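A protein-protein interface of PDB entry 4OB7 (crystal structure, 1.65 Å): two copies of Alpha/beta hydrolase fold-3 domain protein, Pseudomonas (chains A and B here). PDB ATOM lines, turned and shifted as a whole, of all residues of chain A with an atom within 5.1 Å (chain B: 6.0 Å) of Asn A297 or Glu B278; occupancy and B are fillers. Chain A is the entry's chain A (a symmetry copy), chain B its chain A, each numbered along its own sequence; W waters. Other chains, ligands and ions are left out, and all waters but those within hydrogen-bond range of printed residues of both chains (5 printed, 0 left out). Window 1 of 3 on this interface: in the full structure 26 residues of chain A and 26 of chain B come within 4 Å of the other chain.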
ATOM      1  N   GLU A 269      22.834   9.222  20.545  1.00  0.00           N
ATOM      2  CA  GLU A 269      22.625  10.608  20.136  1.00  0.00           C
ATOM      3  C   GLU A 269      23.672  11.562  20.721  1.00  0.00           C
ATOM      4  O   GLU A 269      24.189  12.432  20.018  1.00  0.00           O
ATOM      5  CB  GLU A 269      21.209  11.081  20.505  1.00  0.00           C
ATOM      6  CG  GLU A 269      20.983  12.562  20.236  1.00  0.00           C
ATOM      7  CD  GLU A 269      19.590  13.029  20.594  1.00  0.00           C
ATOM      8  OE1 GLU A 269      18.903  12.341  21.377  1.00  0.00           O
ATOM      9  OE2 GLU A 269      19.174  14.096  20.091  1.00  0.00           O
ATOM     10  N   PHE A 270      23.977  11.402  22.006  1.00  0.00           N
ATOM     11  CA  PHE A 270      24.875  12.337  22.695  1.00  0.00           C
ATOM     12  C   PHE A 270      26.249  11.727  22.882  1.00  0.00           C
ATOM     13  O   PHE A 270      26.649  11.385  23.999  1.00  0.00           O
ATOM     14  CB  PHE A 270      24.275  12.726  24.046  1.00  0.00           C
ATOM     15  CG  PHE A 270      22.983  13.473  23.922  1.00  0.00           C
ATOM     16  CD1 PHE A 270      22.986  14.838  23.702  1.00  0.00           C
ATOM     17  CD2 PHE A 270      21.763  12.808  23.991  1.00  0.00           C
ATOM     18  CE1 PHE A 270      21.800  15.535  23.562  1.00  0.00           C
ATOM     19  CE2 PHE A 270      20.568  13.496  23.852  1.00  0.00           C
ATOM     20  CZ  PHE A 270      20.586  14.867  23.636  1.00  0.00           C
ATOM     21  N   ARG A 295      19.908   5.115  15.584  1.00  0.00           N
ATOM     22  CA  ARG A 295      20.397   6.061  16.575  1.00  0.00           C
ATOM     23  C   ARG A 295      19.486   6.001  17.797  1.00  0.00           C
ATOM     24  O   ARG A 295      18.279   6.263  17.702  1.00  0.00           O
ATOM     25  CB  ARG A 295      20.408   7.485  16.001  1.00  0.00           C
ATOM     26  CG  ARG A 295      20.795   8.568  17.028  1.00  0.00           C
ATOM     27  CD  ARG A 295      20.538   9.972  16.475  1.00  0.00           C
ATOM     28  NE  ARG A 295      21.462  10.318  15.393  1.00  0.00           N
ATOM     29  CZ  ARG A 295      21.629  11.551  14.926  1.00  0.00           C
ATOM     30  NH1 ARG A 295      20.931  12.560  15.440  1.00  0.00           N
ATOM     31  NH2 ARG A 295      22.506  11.782  13.959  1.00  0.00           N
ATOM     32  N   TYR A 296      20.060   5.648  18.942  1.00  0.00           N
ATOM     33  CA  TYR A 296      19.303   5.679  20.190  1.00  0.00           C
ATOM     34  C   TYR A 296      19.361   7.062  20.792  1.00  0.00           C
ATOM     35  O   TYR A 296      20.386   7.494  21.318  1.00  0.00           O
ATOM     36  CB  TYR A 296      19.790   4.602  21.166  1.00  0.00           C
ATOM     37  CG  TYR A 296      19.151   3.281  20.839  1.00  0.00           C
ATOM     38  CD1 TYR A 296      19.558   2.553  19.729  1.00  0.00           C
ATOM     39  CD2 TYR A 296      18.102   2.792  21.604  1.00  0.00           C
ATOM     40  CE1 TYR A 296      18.942   1.353  19.399  1.00  0.00           C
ATOM     41  CE2 TYR A 296      17.493   1.590  21.292  1.00  0.00           C
ATOM     42  CZ  TYR A 296      17.917   0.884  20.188  1.00  0.00           C
ATOM     43  OH  TYR A 296      17.311  -0.303  19.855  1.00  0.00           O
ATOM     44  N   ASN A 297      18.244   7.762  20.690  1.00  0.00           N
ATOM     45  CA  ASN A 297      18.177   9.122  21.172  1.00  0.00           C
ATOM     46  C   ASN A 297      18.213   9.161  22.696  1.00  0.00           C
ATOM     47  O   ASN A 297      17.828   8.196  23.363  1.00  0.00           O
ATOM     48  CB  ASN A 297      16.923   9.795  20.608  1.00  0.00           C
ATOM     49  CG  ASN A 297      17.027  10.023  19.112  1.00  0.00           C
ATOM     50  OD1 ASN A 297      18.110  10.319  18.600  1.00  0.00           O
ATOM     51  ND2 ASN A 297      15.915   9.870  18.402  1.00  0.00           N
ATOM     52  N   GLY A 298      18.707  10.267  23.243  1.00  0.00           N
ATOM     53  CA  GLY A 298      18.798  10.419  24.687  1.00  0.00           C
ATOM     54  C   GLY A 298      19.975   9.712  25.343  1.00  0.00           C
ATOM     55  O   GLY A 298      20.232   9.916  26.533  1.00  0.00           O
ATOM     56  N   MET A 299      20.689   8.881  24.583  1.00  0.00           N
ATOM     57  CA  MET A 299      21.740   8.041  25.151  1.00  0.00           C
ATOM     58  C   MET A 299      23.113   8.675  25.054  1.00  0.00           C
ATOM     59  O   MET A 299      23.385   9.443  24.137  1.00  0.00           O
ATOM     60  CB  MET A 299      21.791   6.681  24.433  1.00  0.00           C
ATOM     61  CG  MET A 299      20.516   5.840  24.526  1.00  0.00           C
ATOM     62  SD  MET A 299      20.114   5.236  26.183  1.00  0.00           S
ATOM     63  CE  MET A 299      18.998   6.508  26.749  1.00  0.00           C
ATOM     64  N   VAL B 265       9.116   5.524  20.481  1.00  0.00           N
ATOM     65  CA  VAL B 265       8.925   6.369  19.316  1.00  0.00           C
ATOM     66  C   VAL B 265       9.994   6.003  18.306  1.00  0.00           C
ATOM     67  O   VAL B 265      11.178   6.167  18.580  1.00  0.00           O
ATOM     68  CB  VAL B 265       9.053   7.856  19.678  1.00  0.00           C
ATOM     69  CG1 VAL B 265       8.761   8.716  18.458  1.00  0.00           C
ATOM     70  CG2 VAL B 265       8.109   8.199  20.829  1.00  0.00           C
ATOM     71  N   THR B 267      11.484   6.948  14.661  1.00  0.00           N
ATOM     72  CA  THR B 267      11.419   7.947  13.596  1.00  0.00           C
ATOM     73  C   THR B 267      12.247   7.482  12.408  1.00  0.00           C
ATOM     74  O   THR B 267      13.066   6.576  12.527  1.00  0.00           O
ATOM     75  CB  THR B 267      11.926   9.324  14.058  1.00  0.00           C
ATOM     76  OG1 THR B 267      13.212   9.173  14.669  1.00  0.00           O
ATOM     77  CG2 THR B 267      10.952   9.967  15.057  1.00  0.00           C
ATOM     78  N   ALA B 268      12.003   8.088  11.252  1.00  0.00           N
ATOM     79  CA  ALA B 268      12.772   7.789  10.049  1.00  0.00           C
ATOM     80  C   ALA B 268      13.726   8.937   9.755  1.00  0.00           C
ATOM     81  O   ALA B 268      13.345  10.098   9.868  1.00  0.00           O
ATOM     82  CB  ALA B 268      11.829   7.569   8.876  1.00  0.00           C
ATOM     83  N   LEU B 273       8.680  14.529   8.952  1.00  0.00           N
ATOM     84  CA  LEU B 273       8.127  14.448  10.300  1.00  0.00           C
ATOM     85  C   LEU B 273       9.135  14.010  11.350  1.00  0.00           C
ATOM     86  O   LEU B 273       8.797  13.917  12.530  1.00  0.00           O
ATOM     87  CB  LEU B 273       6.947  13.471  10.332  1.00  0.00           C
ATOM     88  CG  LEU B 273       5.832  13.758   9.336  1.00  0.00           C
ATOM     89  CD1 LEU B 273       4.819  12.647   9.406  1.00  0.00           C
ATOM     90  CD2 LEU B 273       5.187  15.087   9.665  1.00  0.00           C
ATOM     91  N   ARG B 274      10.363  13.717  10.928  1.00  0.00           N
ATOM     92  CA  ARG B 274      11.371  13.201  11.845  1.00  0.00           C
ATOM     93  C   ARG B 274      11.552  14.102  13.054  1.00  0.00           C
ATOM     94  O   ARG B 274      11.479  13.643  14.192  1.00  0.00           O
ATOM     95  CB  ARG B 274      12.711  13.040  11.127  1.00  0.00           C
ATOM     96  CG  ARG B 274      13.839  12.538  12.021  1.00  0.00           C
ATOM     97  CD  ARG B 274      15.158  12.704  11.286  1.00  0.00           C
ATOM     98  NE  ARG B 274      15.583  14.103  11.292  1.00  0.00           N
ATOM     99  CZ  ARG B 274      16.538  14.600  10.520  1.00  0.00           C
ATOM    100  NH1 ARG B 274      17.157  13.820   9.648  1.00  0.00           N
ATOM    101  NH2 ARG B 274      16.866  15.884  10.617  1.00  0.00           N
ATOM    102  N   ASP B 275      11.765  15.391  12.817  1.00  0.00           N
ATOM    103  CA  ASP B 275      12.128  16.273  13.918  1.00  0.00           C
ATOM    104  C   ASP B 275      11.006  16.463  14.939  1.00  0.00           C
ATOM    105  O   ASP B 275      11.267  16.501  16.144  1.00  0.00           O
ATOM    106  CB  ASP B 275      12.628  17.629  13.399  1.00  0.00           C
ATOM    107  CG  ASP B 275      14.005  17.544  12.768  1.00  0.00           C
ATOM    108  OD1 ASP B 275      14.606  16.450  12.752  1.00  0.00           O
ATOM    109  OD2 ASP B 275      14.511  18.591  12.303  1.00  0.00           O
ATOM    110  N   GLU B 276       9.765  16.579  14.473  1.00  0.00           N
ATOM    111  CA  GLU B 276       8.669  16.776  15.413  1.00  0.00           C
ATOM    112  C   GLU B 276       8.400  15.503  16.212  1.00  0.00           C
ATOM    113  O   GLU B 276       7.932  15.566  17.346  1.00  0.00           O
ATOM    114  CB  GLU B 276       7.391  17.259  14.710  1.00  0.00           C
ATOM    115  CG  GLU B 276       6.701  16.221  13.846  1.00  0.00           C
ATOM    116  CD  GLU B 276       5.732  16.860  12.879  1.00  0.00           C
ATOM    117  OE1 GLU B 276       6.190  17.681  12.051  1.00  0.00           O
ATOM    118  OE2 GLU B 276       4.518  16.564  12.945  1.00  0.00           O
ATOM    119  N   GLY B 277       8.698  14.348  15.620  1.00  0.00           N
ATOM    120  CA  GLY B 277       8.555  13.091  16.340  1.00  0.00           C
ATOM    121  C   GLY B 277       9.602  12.995  17.438  1.00  0.00           C
ATOM    122  O   GLY B 277       9.305  12.619  18.579  1.00  0.00           O
ATOM    123  N   GLU B 278      10.845  13.324  17.094  1.00  0.00           N
ATOM    124  CA  GLU B 278      11.913  13.293  18.084  1.00  0.00           C
ATOM    125  C   GLU B 278      11.716  14.373  19.142  1.00  0.00           C
ATOM    126  O   GLU B 278      12.055  14.171  20.311  1.00  0.00           O
ATOM    127  CB  GLU B 278      13.285  13.385  17.410  1.00  0.00           C
ATOM    128  CG  GLU B 278      13.509  12.209  16.481  1.00  0.00           C
ATOM    129  CD  GLU B 278      14.894  12.140  15.897  1.00  0.00           C
ATOM    130  OE1 GLU B 278      15.663  13.114  16.021  1.00  0.00           O
ATOM    131  OE2 GLU B 278      15.208  11.099  15.294  1.00  0.00           O
ATOM    132  N   ALA B 279      11.156  15.511  18.739  1.00  0.00           N
ATOM    133  CA  ALA B 279      10.882  16.586  19.685  1.00  0.00           C
ATOM    134  C   ALA B 279       9.809  16.165  20.678  1.00  0.00           C
ATOM    135  O   ALA B 279       9.893  16.500  21.856  1.00  0.00           O
ATOM    136  CB  ALA B 279      10.466  17.858  18.959  1.00  0.00           C
ATOM    137  N   TYR B 280       8.810  15.417  20.211  1.00  0.00           N
ATOM    138  CA  TYR B 280       7.755  14.953  21.110  1.00  0.00           C
ATOM    139  C   TYR B 280       8.329  13.951  22.108  1.00  0.00           C
ATOM    140  O   TYR B 280       7.993  13.981  23.292  1.00  0.00           O
ATOM    141  CB  TYR B 280       6.576  14.355  20.331  1.00  0.00           C
ATOM    142  CG  TYR B 280       5.395  14.020  21.212  1.00  0.00           C
ATOM    143  CD1 TYR B 280       4.729  15.021  21.907  1.00  0.00           C
ATOM    144  CD2 TYR B 280       4.943  12.715  21.346  1.00  0.00           C
ATOM    145  CE1 TYR B 280       3.648  14.737  22.714  1.00  0.00           C
ATOM    146  CE2 TYR B 280       3.854  12.417  22.164  1.00  0.00           C
ATOM    147  CZ  TYR B 280       3.217  13.441  22.844  1.00  0.00           C
ATOM    148  OH  TYR B 280       2.139  13.170  23.651  1.00  0.00           O
ATOM    149  N   ALA B 281       9.222  13.082  21.641  1.00  0.00           N
ATOM    150  CA  ALA B 281       9.893  12.161  22.553  1.00  0.00           C
ATOM    151  C   ALA B 281      10.665  12.924  23.633  1.00  0.00           C
ATOM    152  O   ALA B 281      10.653  12.536  24.804  1.00  0.00           O
ATOM    153  CB  ALA B 281      10.830  11.223  21.786  1.00  0.00           C
ATOM    154  N   ARG B 282      11.346  14.000  23.247  1.00  0.00           N
ATOM    155  CA  ARG B 282      12.065  14.815  24.227  1.00  0.00           C
ATOM    156  C   ARG B 282      11.119  15.465  25.232  1.00  0.00           C
ATOM    157  O   ARG B 282      11.437  15.557  26.413  1.00  0.00           O
ATOM    158  CB  ARG B 282      12.904  15.903  23.552  1.00  0.00           C
ATOM    159  CG  ARG B 282      14.155  15.401  22.848  1.00  0.00           C
ATOM    160  CD  ARG B 282      15.039  16.582  22.487  1.00  0.00           C
ATOM    161  NE  ARG B 282      16.327  16.171  21.929  1.00  0.00           N
ATOM    162  CZ  ARG B 282      17.284  17.026  21.570  1.00  0.00           C
ATOM    163  NH1 ARG B 282      17.091  18.328  21.707  1.00  0.00           N
ATOM    164  NH2 ARG B 282      18.431  16.579  21.075  1.00  0.00           N
ATOM    165  N   LYS B 283       9.963  15.927  24.767  1.00  0.00           N
ATOM    166  CA  LYS B 283       8.995  16.524  25.684  1.00  0.00           C
ATOM    167  C   LYS B 283       8.451  15.503  26.676  1.00  0.00           C
ATOM    168  O   LYS B 283       8.263  15.815  27.847  1.00  0.00           O
ATOM    169  CB  LYS B 283       7.847  17.193  24.928  1.00  0.00           C
ATOM    170  CG  LYS B 283       8.201  18.570  24.395  1.00  0.00           C
ATOM    171  CD  LYS B 283       6.940  19.390  24.176  1.00  0.00           C
ATOM    172  CE  LYS B 283       7.084  20.816  24.692  1.00  0.00           C
ATOM    173  NZ  LYS B 283       5.895  21.654  24.333  1.00  0.00           N
ATOM    174  N   THR B 292      11.628   5.480  24.948  1.00  0.00           N
ATOM    175  CA  THR B 292      12.703   4.972  24.111  1.00  0.00           C
ATOM    176  C   THR B 292      12.468   5.616  22.755  1.00  0.00           C
ATOM    177  O   THR B 292      11.398   5.450  22.165  1.00  0.00           O
ATOM    178  CB  THR B 292      12.633   3.435  24.003  1.00  0.00           C
ATOM    179  OG1 THR B 292      12.764   2.869  25.315  1.00  0.00           O
ATOM    180  CG2 THR B 292      13.766   2.886  23.116  1.00  0.00           C
ATOM    181  N   SER B 293      13.442   6.389  22.286  1.00  0.00           N
ATOM    182  CA  SER B 293      13.302   7.112  21.031  1.00  0.00           C
ATOM    183  C   SER B 293      14.433   6.641  20.123  1.00  0.00           C
ATOM    184  O   SER B 293      15.607   6.798  20.456  1.00  0.00           O
ATOM    185  CB  SER B 293      13.394   8.616  21.285  1.00  0.00           C
ATOM    186  OG  SER B 293      13.446   9.337  20.066  1.00  0.00           O
ATOM    187  N   VAL B 294      14.078   6.043  18.987  1.00  0.00           N
ATOM    188  CA  VAL B 294      15.061   5.440  18.085  1.00  0.00           C
ATOM    189  C   VAL B 294      14.856   5.951  16.663  1.00  0.00           C
ATOM    190  O   VAL B 294      13.769   5.810  16.108  1.00  0.00           O
ATOM    191  CB  VAL B 294      14.939   3.891  18.064  1.00  0.00           C
ATOM    192  CG1 VAL B 294      16.062   3.273  17.250  1.00  0.00           C
ATOM    193  CG2 VAL B 294      14.951   3.325  19.473  1.00  0.00           C
ATOM    194  N   ARG B 295      15.897   6.547  16.083  1.00  0.00           N
ATOM    195  CA  ARG B 295      15.857   6.997  14.700  1.00  0.00           C
ATOM    196  C   ARG B 295      16.388   5.878  13.810  1.00  0.00           C
ATOM    197  O   ARG B 295      17.540   5.447  13.951  1.00  0.00           O
ATOM    198  CB  ARG B 295      16.712   8.259  14.518  1.00  0.00           C
ATOM    199  CG  ARG B 295      16.825   8.730  13.055  1.00  0.00           C
ATOM    200  CD  ARG B 295      17.887   9.822  12.906  1.00  0.00           C
ATOM    201  NE  ARG B 295      17.480  11.079  13.537  1.00  0.00           N
ATOM    202  CZ  ARG B 295      18.085  12.244  13.329  1.00  0.00           C
ATOM    203  NH1 ARG B 295      19.131  12.316  12.511  1.00  0.00           N
ATOM    204  NH2 ARG B 295      17.636  13.341  13.924  1.00  0.00           N
HETATM  205  O   HOH W   1      20.882  10.166  11.548  1.00  0.00           O
HETATM  206  O   HOH W   2      16.265  13.384  19.459  1.00  0.00           O
HETATM  207  O   HOH W   3      18.464  12.486  17.029  1.00  0.00           O
HETATM  208  O   HOH W   4      16.919  13.447  22.706  1.00  0.00           O
HETATM  209  O   HOH W   5      15.650   6.686  23.958  1.00  0.00           O
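The backbone carbonyl oxygen of Ser B293 is in hydrogen-bond range of the backbone NH of Asn A297, at 2.8 Å.
O of Arg A295 is in hydrogen-bond range of N of Arg B295, 2.9 Å away.
The side-chain carboxylate (OE2) of Glu B278 sits at hydrogen-bond distance from the side-chain amide nitrogen (ND2) of Asn A297 (3.4 Å).
OE2 of Glu A269 is in salt-bridge range of NH2 of Arg B282, 2.8 Å away.
The backbone NH of Thr B267 lies within hydrogen-bond range of the backbone carbonyl oxygen of Val B294, at 2.9 Å.
The side-chain hydroxyl (OG1) of Thr B267 lies within hydrogen-bond range of the side-chain carboxylate (OE2) of Glu B278, 2.8 Å away.
The backbone NH (N) of Phe A270 lies within hydrogen-bond range of the backbone carbonyl oxygen (O) of Met A299.
The side-chain carboxylate of Glu A269 lies within hydrogen-bond range of the backbone NH of Gly A298 (2.8 Å).
The backbone carbonyl oxygen (O) of Val B265 lies within hydrogen-bond range of the backbone NH (N) of Val B294 (2.9 Å).
O of Tyr A296 sits at hydrogen-bond distance from N of Glu A269, 3.1 Å away.
Among the printed residues, pairs that only touch across the chains: Phe A270 with Arg B282 (3.8 Å), Arg A295 with Ser B293 (3.9 Å), Arg A295 with Val B294 (3.3 Å), Tyr A296 with Ser B293 (3.8 Å) and Tyr A296 with Val B294 (3.6 Å).
Asn A297 touches just these residues of chain B: Glu B278 and Ser B293.
Of the printed residues of chain A, Arg B295 touches Arg A295.
Of the printed residues of chain A, Ser B293 touches Arg A295 (3.9 Å), Tyr A296 (3.8 Å) and Asn A297 (2.8 Å).
Printed residues of chain B within 4 Å of Tyr A296: Ser B293 and Val B294.
Val B265 touches none of the printed residues of chain A.
Ala B279 touches none of the printed residues of chain A.
Of the 18 printed residues of chain B, 5 touch a printed residue of chain A.
Printed residues of chain A that touch a printed residue of chain B: Glu A269, Phe A270, Arg A295, Tyr A296 and Asn A297.
Hydrophobic or aromatic side chains of chain A within 4 Å of the printed part of chain B: Phe A270 and Tyr A296.
Among the printed residues, 9 pairs touch across the chains.
Among the printed residues, Asp or Glu carboxylates within 4 Å of a Lys or Arg side-chain nitrogen of the other chain: Glu A269 with Arg B282.
Arg B295 touches its own counterpart, Arg A295.
Water W4 lies within hydrogen-bond range of OE1 of Glu A269 and NE of Arg B282.
Water W3 lies within hydrogen-bond range of the side-chain amide oxygen of Asn A297 (2.7 Å), the guanidinium group of Arg A295 (2.9 Å), the side-chain carboxylate of Glu B278 (3.0 Å) and the guanidinium group of Arg B295 (3.3 Å).
Water W5 lies within hydrogen-bond range of the backbone carbonyl oxygen of Asn A297 (2.7 Å) and the backbone NH of Ser B293 (2.8 Å).
Water W1 lies within hydrogen-bond range of the guanidinium group of Arg B295 (2.9 Å) and the guanidinium group of Arg A295 (3.3 Å).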
